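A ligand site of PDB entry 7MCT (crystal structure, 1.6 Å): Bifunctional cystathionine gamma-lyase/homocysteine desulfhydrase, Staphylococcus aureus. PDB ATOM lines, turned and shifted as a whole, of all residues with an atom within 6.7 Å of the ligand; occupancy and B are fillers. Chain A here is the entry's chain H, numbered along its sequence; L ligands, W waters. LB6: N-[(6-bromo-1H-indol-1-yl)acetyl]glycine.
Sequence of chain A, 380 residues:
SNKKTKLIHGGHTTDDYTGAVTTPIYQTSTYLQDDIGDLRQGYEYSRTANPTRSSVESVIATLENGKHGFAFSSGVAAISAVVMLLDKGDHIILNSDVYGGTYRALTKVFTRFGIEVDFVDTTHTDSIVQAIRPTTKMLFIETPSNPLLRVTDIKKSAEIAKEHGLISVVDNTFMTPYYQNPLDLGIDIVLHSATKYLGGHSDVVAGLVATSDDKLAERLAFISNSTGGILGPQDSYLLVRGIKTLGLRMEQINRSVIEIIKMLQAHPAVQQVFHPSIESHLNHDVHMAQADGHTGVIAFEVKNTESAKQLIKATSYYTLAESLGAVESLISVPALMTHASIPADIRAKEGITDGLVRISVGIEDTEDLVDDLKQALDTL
CE2 of Tyr 103 touches C2 of the ligand, 3.1 Å away.
NE2 of His 339 touches C12 of the ligand, 3.2 Å away.
Ile 342 touches the ligand.
CG2 of Ile 346 touches C5 of the ligand (3.9 Å).
CG of Glu 350 touches BR of the ligand, 3.3 Å away.
Ile 352 touches the ligand (CG1 to BR, 3.9 Å).
Within 4 Å of the ligand: Gly 100, Tyr 103, Thr 338, His 339, Ile 342, Ile 346, Glu 350 and Ile 352.
Along chain A the residues within 4 Å of the ligand span positions 100 to 352.
A ring nitrogen (ND1) of His 339 lies within hydrogen-bond range of the side-chain hydroxyl (OG1) of Thr 338.
O of Tyr 103 lies within hydrogen-bond range of OG1 of Thr 107, 2.7 Å away.
The backbone carbonyl oxygen (O) of Ile 342 is in hydrogen-bond range of the guanidinium group (NH1) of Arg 347, 2.7 Å away.
The backbone carbonyl oxygen of Arg 347 lies within hydrogen-bond range of the backbone NH of Ile 352, at 2.9 Å.
Water W2 lies within hydrogen-bond range of O2 of the ligand (2.6 Å), ND2 of Asn 146 (2.9 Å) and N of Gly 100 (3.4 Å).
The backbone carbonyl oxygen (O) of Thr 338 sits close to an oxygen (O3) of the ligand (2.8 Å).
The backbone NH of Gly 100 is in hydrogen-bond range of an oxygen (O2) of the ligand.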
ATOM      1  N   SER A  96       9.091  18.713 -13.850  1.00  0.00           N
ATOM      2  CA  SER A  96       8.828  17.514 -14.631  1.00  0.00           C
ATOM      3  C   SER A  96       8.765  17.793 -16.117  1.00  0.00           C
ATOM      4  O   SER A  96       9.141  16.935 -16.931  1.00  0.00           O
ATOM      5  CB  SER A  96       7.516  16.855 -14.169  1.00  0.00           C
ATOM      6  OG  SER A  96       6.440  17.777 -14.235  1.00  0.00           O
ATOM      7  N   ASP A  97       8.290  18.972 -16.498  1.00  0.00           N
ATOM      8  CA  ASP A  97       8.011  19.289 -17.898  1.00  0.00           C
ATOM      9  C   ASP A  97       9.001  20.314 -18.456  1.00  0.00           C
ATOM     10  O   ASP A  97       8.639  21.184 -19.240  1.00  0.00           O
ATOM     11  CB  ASP A  97       6.588  19.799 -18.058  1.00  0.00           C
ATOM     12  CG  ASP A  97       6.263  20.958 -17.143  1.00  0.00           C
ATOM     13  OD1 ASP A  97       7.115  21.328 -16.305  1.00  0.00           O
ATOM     14  OD2 ASP A  97       5.142  21.515 -17.247  1.00  0.00           O
ATOM     15  N   VAL A  98      10.273  20.192 -18.063  1.00  0.00           N
ATOM     16  CA  VAL A  98      11.297  21.144 -18.507  1.00  0.00           C
ATOM     17  C   VAL A  98      11.419  21.144 -20.040  1.00  0.00           C
ATOM     18  O   VAL A  98      11.070  20.175 -20.722  1.00  0.00           O
ATOM     19  CB  VAL A  98      12.629  20.786 -17.823  1.00  0.00           C
ATOM     20  CG1 VAL A  98      13.330  19.636 -18.544  1.00  0.00           C
ATOM     21  CG2 VAL A  98      13.530  22.012 -17.726  1.00  0.00           C
ATOM     22  N   TYR A  99      11.905  22.275 -20.571  1.00  0.00           N
ATOM     23  CA  TYR A  99      12.109  22.444 -21.999  1.00  0.00           C
ATOM     24  C   TYR A  99      12.820  21.239 -22.612  1.00  0.00           C
ATOM     25  O   TYR A  99      13.764  20.695 -22.034  1.00  0.00           O
ATOM     26  CB  TYR A  99      12.917  23.719 -22.234  1.00  0.00           C
ATOM     27  CG  TYR A  99      13.432  23.919 -23.643  1.00  0.00           C
ATOM     28  CD1 TYR A  99      12.557  24.159 -24.692  1.00  0.00           C
ATOM     29  CD2 TYR A  99      14.795  23.898 -23.909  1.00  0.00           C
ATOM     30  CE1 TYR A  99      13.025  24.361 -25.976  1.00  0.00           C
ATOM     31  CE2 TYR A  99      15.276  24.088 -25.194  1.00  0.00           C
ATOM     32  CZ  TYR A  99      14.389  24.322 -26.216  1.00  0.00           C
ATOM     33  OH  TYR A  99      14.867  24.518 -27.493  1.00  0.00           O
ATOM     34  N   GLY A 100      12.354  20.820 -23.796  1.00  0.00           N
ATOM     35  CA  GLY A 100      12.879  19.621 -24.418  1.00  0.00           C
ATOM     36  C   GLY A 100      14.380  19.640 -24.623  1.00  0.00           C
ATOM     37  O   GLY A 100      15.052  18.618 -24.451  1.00  0.00           O
ATOM     38  N   GLY A 101      14.933  20.797 -25.000  1.00  0.00           N
ATOM     39  CA  GLY A 101      16.378  20.889 -25.134  1.00  0.00           C
ATOM     40  C   GLY A 101      17.105  20.687 -23.813  1.00  0.00           C
ATOM     41  O   GLY A 101      18.175  20.075 -23.772  1.00  0.00           O
ATOM     42  N   TYR A 103      15.880  18.885 -21.276  1.00  0.00           N
ATOM     43  CA  TYR A 103      15.735  17.456 -21.010  1.00  0.00           C
ATOM     44  C   TYR A 103      16.768  16.647 -21.793  1.00  0.00           C
ATOM     45  O   TYR A 103      17.406  15.745 -21.247  1.00  0.00           O
ATOM     46  CB  TYR A 103      14.312  17.006 -21.360  1.00  0.00           C
ATOM     47  CG  TYR A 103      14.111  15.517 -21.195  1.00  0.00           C
ATOM     48  CD1 TYR A 103      13.779  14.980 -19.957  1.00  0.00           C
ATOM     49  CD2 TYR A 103      14.274  14.646 -22.268  1.00  0.00           C
ATOM     50  CE1 TYR A 103      13.602  13.615 -19.800  1.00  0.00           C
ATOM     51  CE2 TYR A 103      14.109  13.277 -22.117  1.00  0.00           C
ATOM     52  CZ  TYR A 103      13.769  12.776 -20.881  1.00  0.00           C
ATOM     53  OH  TYR A 103      13.599  11.419 -20.715  1.00  0.00           O
ATOM     54  N   ARG A 104      16.931  16.965 -23.087  1.00  0.00           N
ATOM     55  CA  ARG A 104      17.872  16.230 -23.938  1.00  0.00           C
ATOM     56  C   ARG A 104      19.301  16.417 -23.471  1.00  0.00           C
ATOM     57  O   ARG A 104      20.073  15.451 -23.375  1.00  0.00           O
ATOM     58  CB  ARG A 104      17.760  16.698 -25.386  1.00  0.00           C
ATOM     59  CG  ARG A 104      16.549  16.238 -26.162  1.00  0.00           C
ATOM     60  CD  ARG A 104      16.681  16.653 -27.639  1.00  0.00           C
ATOM     61  NE  ARG A 104      16.840  18.103 -27.813  1.00  0.00           N
ATOM     62  CZ  ARG A 104      17.965  18.711 -28.178  1.00  0.00           C
ATOM     63  NH1 ARG A 104      19.055  17.996 -28.438  1.00  0.00           N
ATOM     64  NH2 ARG A 104      18.002  20.036 -28.296  1.00  0.00           N
ATOM     65  N   THR A 107      19.702  14.389 -20.130  1.00  0.00           N
ATOM     66  CA  THR A 107      19.559  12.931 -20.149  1.00  0.00           C
ATOM     67  C   THR A 107      20.393  12.242 -21.219  1.00  0.00           C
ATOM     68  O   THR A 107      20.612  11.027 -21.118  1.00  0.00           O
ATOM     69  CB  THR A 107      18.094  12.521 -20.324  1.00  0.00           C
ATOM     70  OG1 THR A 107      17.582  13.039 -21.570  1.00  0.00           O
ATOM     71  CG2 THR A 107      17.239  13.024 -19.162  1.00  0.00           C
ATOM     72  N   ASN A 146       6.592  24.949 -20.392  1.00  0.00           N
ATOM     73  CA  ASN A 146       6.091  24.772 -21.750  1.00  0.00           C
ATOM     74  C   ASN A 146       5.641  23.331 -21.988  1.00  0.00           C
ATOM     75  O   ASN A 146       6.328  22.401 -21.535  1.00  0.00           O
ATOM     76  CB  ASN A 146       7.180  25.138 -22.765  1.00  0.00           C
ATOM     77  CG  ASN A 146       6.698  25.003 -24.187  1.00  0.00           C
ATOM     78  OD1 ASN A 146       5.877  25.805 -24.650  1.00  0.00           O
ATOM     79  ND2 ASN A 146       7.199  24.000 -24.897  1.00  0.00           N
ATOM     80  N   PRO A 147       4.520  23.105 -22.692  1.00  0.00           N
ATOM     81  CA  PRO A 147       3.569  24.071 -23.250  1.00  0.00           C
ATOM     82  C   PRO A 147       2.319  24.266 -22.401  1.00  0.00           C
ATOM     83  O   PRO A 147       1.383  24.927 -22.846  1.00  0.00           O
ATOM     84  CB  PRO A 147       3.194  23.438 -24.594  1.00  0.00           C
ATOM     85  CG  PRO A 147       3.165  21.963 -24.261  1.00  0.00           C
ATOM     86  CD  PRO A 147       4.262  21.749 -23.216  1.00  0.00           C
ATOM     87  N   MET A 337       5.338  18.731 -33.487  1.00  0.00           N
ATOM     88  CA  MET A 337       6.557  19.494 -33.734  1.00  0.00           C
ATOM     89  C   MET A 337       7.609  19.324 -32.658  1.00  0.00           C
ATOM     90  O   MET A 337       8.773  19.075 -32.970  1.00  0.00           O
ATOM     91  CB  MET A 337       6.212  20.980 -33.906  1.00  0.00           C
ATOM     92  CG  MET A 337       5.424  21.234 -35.181  1.00  0.00           C
ATOM     93  SD  MET A 337       4.727  22.887 -35.339  1.00  0.00           S
ATOM     94  CE  MET A 337       6.193  23.922 -35.342  1.00  0.00           C
ATOM     95  N   THR A 338       7.233  19.449 -31.395  1.00  0.00           N
ATOM     96  CA  THR A 338       8.204  19.353 -30.308  1.00  0.00           C
ATOM     97  C   THR A 338       8.124  18.045 -29.552  1.00  0.00           C
ATOM     98  O   THR A 338       9.158  17.566 -29.071  1.00  0.00           O
ATOM     99  CB  THR A 338       8.024  20.526 -29.335  1.00  0.00           C
ATOM    100  OG1 THR A 338       6.682  20.553 -28.836  1.00  0.00           O
ATOM    101  CG2 THR A 338       8.324  21.837 -30.028  1.00  0.00           C
ATOM    102  N   HIS A 339       6.953  17.425 -29.459  1.00  0.00           N
ATOM    103  CA  HIS A 339       6.755  16.209 -28.678  1.00  0.00           C
ATOM    104  C   HIS A 339       6.490  14.986 -29.556  1.00  0.00           C
ATOM    105  O   HIS A 339       5.935  13.999 -29.074  1.00  0.00           O
ATOM    106  CB  HIS A 339       5.622  16.399 -27.675  1.00  0.00           C
ATOM    107  CG  HIS A 339       5.902  17.412 -26.612  1.00  0.00           C
ATOM    108  ND1 HIS A 339       6.005  18.757 -26.880  1.00  0.00           N
ATOM    109  CD2 HIS A 339       6.075  17.275 -25.275  1.00  0.00           C
ATOM    110  CE1 HIS A 339       6.248  19.407 -25.753  1.00  0.00           C
ATOM    111  NE2 HIS A 339       6.286  18.533 -24.770  1.00  0.00           N
ATOM    112  N   ALA A 340       6.900  15.033 -30.832  1.00  0.00           N
ATOM    113  CA  ALA A 340       6.452  14.016 -31.789  1.00  0.00           C
ATOM    114  C   ALA A 340       7.068  12.652 -31.524  1.00  0.00           C
ATOM    115  O   ALA A 340       6.461  11.627 -31.871  1.00  0.00           O
ATOM    116  CB  ALA A 340       6.772  14.477 -33.205  1.00  0.00           C
ATOM    117  N   SER A 341       8.259  12.586 -30.929  1.00  0.00           N
ATOM    118  CA  SER A 341       8.899  11.288 -30.730  1.00  0.00           C
ATOM    119  C   SER A 341       8.335  10.531 -29.540  1.00  0.00           C
ATOM    120  O   SER A 341       8.662   9.349 -29.366  1.00  0.00           O
ATOM    121  CB  SER A 341      10.403  11.462 -30.588  1.00  0.00           C
ATOM    122  OG  SER A 341      10.714  12.342 -29.521  1.00  0.00           O
ATOM    123  N   ILE A 342       7.521  11.175 -28.712  1.00  0.00           N
ATOM    124  CA  ILE A 342       6.900  10.548 -27.557  1.00  0.00           C
ATOM    125  C   ILE A 342       5.700   9.735 -28.020  1.00  0.00           C
ATOM    126  O   ILE A 342       4.926  10.196 -28.882  1.00  0.00           O
ATOM    127  CB  ILE A 342       6.512  11.602 -26.520  1.00  0.00           C
ATOM    128  CG1 ILE A 342       7.775  12.311 -26.038  1.00  0.00           C
ATOM    129  CG2 ILE A 342       5.732  10.950 -25.369  1.00  0.00           C
ATOM    130  CD1 ILE A 342       7.510  13.712 -25.627  1.00  0.00           C
ATOM    131  N   PRO A 343       5.531   8.505 -27.526  1.00  0.00           N
ATOM    132  CA  PRO A 343       4.385   7.689 -27.919  1.00  0.00           C
ATOM    133  C   PRO A 343       3.079   8.431 -27.718  1.00  0.00           C
ATOM    134  O   PRO A 343       2.913   9.199 -26.762  1.00  0.00           O
ATOM    135  CB  PRO A 343       4.501   6.467 -26.989  1.00  0.00           C
ATOM    136  CG  PRO A 343       6.006   6.299 -26.877  1.00  0.00           C
ATOM    137  CD  PRO A 343       6.446   7.746 -26.645  1.00  0.00           C
ATOM    138  N   ILE A 346       1.268   8.182 -24.402  1.00  0.00           N
ATOM    139  CA  ILE A 346       1.935   8.917 -23.339  1.00  0.00           C
ATOM    140  C   ILE A 346       1.730  10.425 -23.524  1.00  0.00           C
ATOM    141  O   ILE A 346       1.507  11.161 -22.549  1.00  0.00           O
ATOM    142  CB  ILE A 346       3.425   8.534 -23.290  1.00  0.00           C
ATOM    143  CG1 ILE A 346       3.564   7.109 -22.740  1.00  0.00           C
ATOM    144  CG2 ILE A 346       4.216   9.499 -22.410  1.00  0.00           C
ATOM    145  CD1 ILE A 346       4.746   6.338 -23.302  1.00  0.00           C
ATOM    146  N   ARG A 347       1.776  10.905 -24.768  1.00  0.00           N
ATOM    147  CA  ARG A 347       1.414  12.289 -25.036  1.00  0.00           C
ATOM    148  C   ARG A 347       0.038  12.608 -24.481  1.00  0.00           C
ATOM    149  O   ARG A 347      -0.150  13.599 -23.759  1.00  0.00           O
ATOM    150  CB  ARG A 347       1.454  12.581 -26.539  1.00  0.00           C
ATOM    151  CG  ARG A 347       2.852  12.711 -27.110  1.00  0.00           C
ATOM    152  CD  ARG A 347       2.829  13.536 -28.373  1.00  0.00           C
ATOM    153  NE  ARG A 347       1.859  13.029 -29.335  1.00  0.00           N
ATOM    154  CZ  ARG A 347       2.133  12.157 -30.298  1.00  0.00           C
ATOM    155  NH1 ARG A 347       3.366  11.688 -30.428  1.00  0.00           N
ATOM    156  NH2 ARG A 347       1.183  11.763 -31.134  1.00  0.00           N
ATOM    157  N   GLU A 350      -0.105  12.916 -20.821  1.00  0.00           N
ATOM    158  CA  GLU A 350       0.509  14.136 -20.321  1.00  0.00           C
ATOM    159  C   GLU A 350      -0.274  15.391 -20.698  1.00  0.00           C
ATOM    160  O   GLU A 350       0.158  16.497 -20.346  1.00  0.00           O
ATOM    161  CB  GLU A 350       1.928  14.243 -20.857  1.00  0.00           C
ATOM    162  CG  GLU A 350       2.856  13.174 -20.332  1.00  0.00           C
ATOM    163  CD  GLU A 350       3.206  13.367 -18.877  1.00  0.00           C
ATOM    164  OE1 GLU A 350       3.250  14.532 -18.431  1.00  0.00           O
ATOM    165  OE2 GLU A 350       3.424  12.362 -18.177  1.00  0.00           O
ATOM    166  N   GLY A 351      -1.397  15.260 -21.395  1.00  0.00           N
ATOM    167  CA  GLY A 351      -2.161  16.416 -21.820  1.00  0.00           C
ATOM    168  C   GLY A 351      -1.703  17.022 -23.123  1.00  0.00           C
ATOM    169  O   GLY A 351      -2.273  18.050 -23.536  1.00  0.00           O
ATOM    170  N   ILE A 352      -0.699  16.447 -23.779  1.00  0.00           N
ATOM    171  CA  ILE A 352      -0.252  16.925 -25.080  1.00  0.00           C
ATOM    172  C   ILE A 352      -1.097  16.250 -26.150  1.00  0.00           C
ATOM    173  O   ILE A 352      -0.631  15.358 -26.875  1.00  0.00           O
ATOM    174  CB  ILE A 352       1.248  16.644 -25.295  1.00  0.00           C
ATOM    175  CG1 ILE A 352       2.053  17.046 -24.061  1.00  0.00           C
ATOM    176  CG2 ILE A 352       1.775  17.397 -26.518  1.00  0.00           C
ATOM    177  CD1 ILE A 352       1.881  18.503 -23.676  1.00  0.00           C
HETATM  178  C10 LB6 L   1      10.324  16.182 -22.582  1.00  0.00           C
HETATM  179  C11 LB6 L   1      10.301  16.507 -24.064  1.00  0.00           C
HETATM  180  C12 LB6 L   1       9.370  18.224 -25.511  1.00  0.00           C
HETATM  181  C13 LB6 L   1      10.148  19.237 -26.328  1.00  0.00           C
HETATM  182  C2  LB6 L   1      11.053  13.816 -22.020  1.00  0.00           C
HETATM  183  C3  LB6 L   1      10.441  12.590 -21.788  1.00  0.00           C
HETATM  184  C4  LB6 L   1       7.894  11.951 -21.824  1.00  0.00           C
HETATM  185  C5  LB6 L   1       6.626  12.492 -22.037  1.00  0.00           C
HETATM  186  C6  LB6 L   1       6.494  13.842 -22.340  1.00  0.00           C
HETATM  187  C7  LB6 L   1       7.582  14.640 -22.435  1.00  0.00           C
HETATM  188  C8  LB6 L   1       8.838  14.113 -22.235  1.00  0.00           C
HETATM  189  C9  LB6 L   1       9.018  12.774 -21.926  1.00  0.00           C
HETATM  190  N1  LB6 L   1      10.074  14.745 -22.292  1.00  0.00           N
HETATM  191  N2  LB6 L   1      10.143  17.792 -24.365  1.00  0.00           N
HETATM  192  O1  LB6 L   1      10.417  15.623 -24.899  1.00  0.00           O
HETATM  193  O2  LB6 L   1      10.009  20.457 -26.090  1.00  0.00           O
HETATM  194  O3  LB6 L   1      10.918  18.817 -27.219  1.00  0.00           O
HETATM  195 BR   LB6 L   1       4.798  14.617 -22.635  1.00  0.00          BR
HETATM  196  O   HOH W   1      12.271  20.279 -28.589  1.00  0.00           O
HETATM  197  O   HOH W   2       9.125  21.955 -24.163  1.00  0.00           O
HETATM  198  O   HOH W   3      10.647  17.460 -19.737  1.00  0.00           O
HETATM  199  O   HOH W   4      13.276  14.116 -25.901  1.00  0.00           O
HETATM  200  O   HOH W   5       9.908  23.387 -27.593  1.00  0.00           O
